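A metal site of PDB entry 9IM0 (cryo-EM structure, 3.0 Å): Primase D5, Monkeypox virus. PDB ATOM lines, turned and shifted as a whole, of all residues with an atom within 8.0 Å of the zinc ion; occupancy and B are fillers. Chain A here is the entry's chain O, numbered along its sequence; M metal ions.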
ATOM      1  N   PHE A 254       5.736   6.298 -18.948  1.00  0.00           N
ATOM      2  CA  PHE A 254       6.192   5.309 -17.981  1.00  0.00           C
ATOM      3  C   PHE A 254       7.158   5.980 -17.014  1.00  0.00           C
ATOM      4  O   PHE A 254       8.260   6.396 -17.408  1.00  0.00           O
ATOM      5  CB  PHE A 254       6.859   4.130 -18.688  1.00  0.00           C
ATOM      6  CG  PHE A 254       5.890   3.141 -19.259  1.00  0.00           C
ATOM      7  CD1 PHE A 254       4.584   3.100 -18.807  1.00  0.00           C
ATOM      8  CD2 PHE A 254       6.294   2.235 -20.227  1.00  0.00           C
ATOM      9  CE1 PHE A 254       3.693   2.182 -19.337  1.00  0.00           C
ATOM     10  CE2 PHE A 254       5.409   1.320 -20.748  1.00  0.00           C
ATOM     11  CZ  PHE A 254       4.109   1.289 -20.303  1.00  0.00           C
ATOM     12  N   TYR A 278      10.741  -2.393 -12.221  1.00  0.00           N
ATOM     13  CA  TYR A 278       9.663  -2.073 -11.295  1.00  0.00           C
ATOM     14  C   TYR A 278      10.232  -1.833  -9.896  1.00  0.00           C
ATOM     15  O   TYR A 278      10.247  -2.708  -9.020  1.00  0.00           O
ATOM     16  CB  TYR A 278       8.621  -3.188 -11.291  1.00  0.00           C
ATOM     17  CG  TYR A 278       7.611  -3.059 -12.406  1.00  0.00           C
ATOM     18  CD1 TYR A 278       6.667  -2.040 -12.400  1.00  0.00           C
ATOM     19  CD2 TYR A 278       7.590  -3.969 -13.453  1.00  0.00           C
ATOM     20  CE1 TYR A 278       5.740  -1.922 -13.419  1.00  0.00           C
ATOM     21  CE2 TYR A 278       6.662  -3.851 -14.472  1.00  0.00           C
ATOM     22  CZ  TYR A 278       5.742  -2.825 -14.446  1.00  0.00           C
ATOM     23  OH  TYR A 278       4.817  -2.716 -15.463  1.00  0.00           O
ATOM     24  N   PRO A 281       5.454   1.546  -8.569  1.00  0.00           N
ATOM     25  CA  PRO A 281       4.297   1.096  -9.361  1.00  0.00           C
ATOM     26  C   PRO A 281       4.152   1.882 -10.650  1.00  0.00           C
ATOM     27  O   PRO A 281       4.467   3.066 -10.719  1.00  0.00           O
ATOM     28  CB  PRO A 281       3.104   1.337  -8.420  1.00  0.00           C
ATOM     29  CG  PRO A 281       3.609   2.307  -7.400  1.00  0.00           C
ATOM     30  CD  PRO A 281       5.051   1.980  -7.216  1.00  0.00           C
ATOM     31  N   CYS A 282       3.674   1.192 -11.688  1.00  0.00           N
ATOM     32  CA  CYS A 282       3.518   1.840 -12.993  1.00  0.00           C
ATOM     33  C   CYS A 282       2.363   2.838 -12.951  1.00  0.00           C
ATOM     34  O   CYS A 282       1.382   2.662 -12.216  1.00  0.00           O
ATOM     35  CB  CYS A 282       3.299   0.804 -14.093  1.00  0.00           C
ATOM     36  SG  CYS A 282       1.622   0.148 -14.320  1.00  0.00           S
ATOM     37  N   ALA A 283       2.490   3.894 -13.745  1.00  0.00           N
ATOM     38  CA  ALA A 283       1.543   5.004 -13.677  1.00  0.00           C
ATOM     39  C   ALA A 283       0.156   4.603 -14.168  1.00  0.00           C
ATOM     40  O   ALA A 283      -0.847   5.168 -13.721  1.00  0.00           O
ATOM     41  CB  ALA A 283       2.062   6.201 -14.466  1.00  0.00           C
ATOM     42  N   LEU A 284       0.080   3.668 -15.117  1.00  0.00           N
ATOM     43  CA  LEU A 284      -1.212   3.264 -15.663  1.00  0.00           C
ATOM     44  C   LEU A 284      -2.103   2.634 -14.587  1.00  0.00           C
ATOM     45  O   LEU A 284      -3.152   3.175 -14.238  1.00  0.00           O
ATOM     46  CB  LEU A 284      -1.008   2.301 -16.830  1.00  0.00           C
ATOM     47  CG  LEU A 284       0.101   2.662 -17.833  1.00  0.00           C
ATOM     48  CD1 LEU A 284       0.113   1.679 -18.989  1.00  0.00           C
ATOM     49  CD2 LEU A 284      -0.072   4.082 -18.342  1.00  0.00           C
ATOM     50  N   CYS A 285      -1.673   1.501 -14.044  1.00  0.00           N
ATOM     51  CA  CYS A 285      -2.345   0.865 -12.918  1.00  0.00           C
ATOM     52  C   CYS A 285      -1.362   0.757 -11.769  1.00  0.00           C
ATOM     53  O   CYS A 285      -0.203   0.380 -11.976  1.00  0.00           O
ATOM     54  CB  CYS A 285      -2.883  -0.522 -13.296  1.00  0.00           C
ATOM     55  SG  CYS A 285      -1.630  -1.832 -13.409  1.00  0.00           S
ATOM     56  N   LYS A 286      -1.800   1.100 -10.562  1.00  0.00           N
ATOM     57  CA  LYS A 286      -0.855   1.153  -9.455  1.00  0.00           C
ATOM     58  C   LYS A 286      -0.293  -0.246  -9.171  1.00  0.00           C
ATOM     59  O   LYS A 286       0.866  -0.519  -9.501  1.00  0.00           O
ATOM     60  CB  LYS A 286      -1.492   1.729  -8.180  1.00  0.00           C
ATOM     61  CG  LYS A 286      -2.057   3.177  -8.213  1.00  0.00           C
ATOM     62  CD  LYS A 286      -2.891   3.567  -9.430  1.00  0.00           C
ATOM     63  CE  LYS A 286      -2.894   5.075  -9.633  1.00  0.00           C
ATOM     64  NZ  LYS A 286      -3.649   5.479 -10.853  1.00  0.00           N
ATOM     65  N   LYS A 287      -1.136  -1.129  -8.642  1.00  0.00           N
ATOM     66  CA  LYS A 287      -0.784  -2.500  -8.276  1.00  0.00           C
ATOM     67  C   LYS A 287       0.626  -2.499  -7.682  1.00  0.00           C
ATOM     68  O   LYS A 287       0.956  -1.616  -6.882  1.00  0.00           O
ATOM     69  CB  LYS A 287      -0.962  -3.415  -9.504  1.00  0.00           C
ATOM     70  CG  LYS A 287      -0.606  -4.894  -9.374  1.00  0.00           C
ATOM     71  CD  LYS A 287      -1.234  -5.732 -10.462  1.00  0.00           C
ATOM     72  CE  LYS A 287      -0.342  -6.901 -10.839  1.00  0.00           C
ATOM     73  NZ  LYS A 287       0.410  -7.424  -9.658  1.00  0.00           N
ATOM     74  N   ARG A 288       1.471  -3.477  -8.034  1.00  0.00           N
ATOM     75  CA  ARG A 288       2.891  -3.453  -7.691  1.00  0.00           C
ATOM     76  C   ARG A 288       3.666  -4.470  -8.527  1.00  0.00           C
ATOM     77  O   ARG A 288       3.433  -5.682  -8.404  1.00  0.00           O
ATOM     78  CB  ARG A 288       3.097  -3.735  -6.201  1.00  0.00           C
ATOM     79  CG  ARG A 288       4.473  -3.342  -5.690  1.00  0.00           C
ATOM     80  CD  ARG A 288       4.646  -1.839  -5.663  1.00  0.00           C
ATOM     81  NE  ARG A 288       6.032  -1.448  -5.944  1.00  0.00           N
ATOM     82  CZ  ARG A 288       6.973  -1.281  -5.021  1.00  0.00           C
ATOM     83  NH1 ARG A 288       6.718  -1.469  -3.735  1.00  0.00           N
ATOM     84  NH2 ARG A 288       8.194  -0.914  -5.400  1.00  0.00           N
ATOM     85  N   SER A 289       4.585  -3.992  -9.365  1.00  0.00           N
ATOM     86  CA  SER A 289       5.591  -4.835 -10.014  1.00  0.00           C
ATOM     87  C   SER A 289       4.941  -5.937 -10.865  1.00  0.00           C
ATOM     88  O   SER A 289       4.997  -7.128 -10.538  1.00  0.00           O
ATOM     89  CB  SER A 289       6.554  -5.427  -8.976  1.00  0.00           C
ATOM     90  OG  SER A 289       7.536  -6.251  -9.604  1.00  0.00           O
ATOM     91  N   HIS A 290       4.286  -5.503 -11.937  1.00  0.00           N
ATOM     92  CA  HIS A 290       3.742  -6.432 -12.920  1.00  0.00           C
ATOM     93  C   HIS A 290       4.784  -7.459 -13.341  1.00  0.00           C
ATOM     94  O   HIS A 290       5.988  -7.183 -13.376  1.00  0.00           O
ATOM     95  CB  HIS A 290       3.252  -5.678 -14.163  1.00  0.00           C
ATOM     96  CG  HIS A 290       2.119  -4.744 -13.903  1.00  0.00           C
ATOM     97  ND1 HIS A 290       1.416  -4.729 -12.727  1.00  0.00           N
ATOM     98  CD2 HIS A 290       1.553  -3.786 -14.689  1.00  0.00           C
ATOM     99  CE1 HIS A 290       0.465  -3.814 -12.784  1.00  0.00           C
ATOM    100  NE2 HIS A 290       0.530  -3.222 -13.968  1.00  0.00           N
ATOM    101  N   HIS A 294       5.308  -5.229 -21.567  1.00  0.00           N
ATOM    102  CA  HIS A 294       4.327  -4.424 -22.282  1.00  0.00           C
ATOM    103  C   HIS A 294       4.624  -4.478 -23.779  1.00  0.00           C
ATOM    104  O   HIS A 294       5.604  -5.069 -24.229  1.00  0.00           O
ATOM    105  CB  HIS A 294       4.342  -2.985 -21.774  1.00  0.00           C
ATOM    106  CG  HIS A 294       3.579  -2.791 -20.502  1.00  0.00           C
ATOM    107  ND1 HIS A 294       3.923  -3.416 -19.327  1.00  0.00           N
ATOM    108  CD2 HIS A 294       2.492  -2.031 -20.225  1.00  0.00           C
ATOM    109  CE1 HIS A 294       3.081  -3.051 -18.375  1.00  0.00           C
ATOM    110  NE2 HIS A 294       2.204  -2.218 -18.896  1.00  0.00           N
ATOM    111  N   LYS A 307      -0.634  -4.454 -22.287  1.00  0.00           N
ATOM    112  CA  LYS A 307       0.143  -5.395 -21.500  1.00  0.00           C
ATOM    113  C   LYS A 307      -0.195  -6.823 -21.902  1.00  0.00           C
ATOM    114  O   LYS A 307      -1.370  -7.187 -22.003  1.00  0.00           O
ATOM    115  CB  LYS A 307      -0.123  -5.194 -20.012  1.00  0.00           C
ATOM    116  CG  LYS A 307       0.251  -6.374 -19.125  1.00  0.00           C
ATOM    117  CD  LYS A 307      -0.169  -6.126 -17.690  1.00  0.00           C
ATOM    118  CE  LYS A 307       0.293  -7.234 -16.767  1.00  0.00           C
ATOM    119  NZ  LYS A 307       1.779  -7.289 -16.668  1.00  0.00           N
ATOM    120  N   SER A 313      -5.661  -6.152 -16.260  1.00  0.00           N
ATOM    121  CA  SER A 313      -4.696  -5.808 -15.219  1.00  0.00           C
ATOM    122  C   SER A 313      -4.229  -4.361 -15.351  1.00  0.00           C
ATOM    123  O   SER A 313      -4.180  -3.628 -14.357  1.00  0.00           O
ATOM    124  CB  SER A 313      -3.507  -6.772 -15.277  1.00  0.00           C
ATOM    125  OG  SER A 313      -3.070  -6.962 -16.619  1.00  0.00           O
ATOM    126  N   CYS A 314      -3.877  -3.939 -16.565  1.00  0.00           N
ATOM    127  CA  CYS A 314      -3.317  -2.614 -16.792  1.00  0.00           C
ATOM    128  C   CYS A 314      -4.212  -1.820 -17.733  1.00  0.00           C
ATOM    129  O   CYS A 314      -4.696  -2.342 -18.740  1.00  0.00           O
ATOM    130  CB  CYS A 314      -1.895  -2.718 -17.382  1.00  0.00           C
ATOM    131  SG  CYS A 314      -0.832  -1.273 -17.080  1.00  0.00           S
ATOM    132  N   LYS A 315      -4.436  -0.550 -17.385  1.00  0.00           N
ATOM    133  CA  LYS A 315      -5.280   0.314 -18.196  1.00  0.00           C
ATOM    134  C   LYS A 315      -4.606   0.640 -19.528  1.00  0.00           C
ATOM    135  O   LYS A 315      -3.379   0.735 -19.625  1.00  0.00           O
ATOM    136  CB  LYS A 315      -5.600   1.604 -17.427  1.00  0.00           C
ATOM    137  CG  LYS A 315      -6.529   2.560 -18.153  1.00  0.00           C
ATOM    138  CD  LYS A 315      -7.889   1.936 -18.398  1.00  0.00           C
ATOM    139  CE  LYS A 315      -8.616   1.670 -17.086  1.00  0.00           C
ATOM    140  NZ  LYS A 315      -9.013   2.932 -16.407  1.00  0.00           N
HETATM  141 ZN    ZN M   1       0.056  -1.467 -14.946  1.00  0.00          ZN
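The side-chain sulfur (SG) of Cys 314 lies close to a ring nitrogen (NE2) of His 294, at 3.7 Å. O of Ser 313 lies close to SG of Cys 285, 3.3 Å away.
Four residues have an atom within 4 Å of the zinc ion: Cys 282, Cys 285, His 290 and Cys 314.
The zinc ion is bound by NE2 of His 290 (2.1 Å), SG of Cys 285 (2.3 Å), SG of Cys 314 (2.3 Å) and SG of Cys 282 (2.3 Å).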
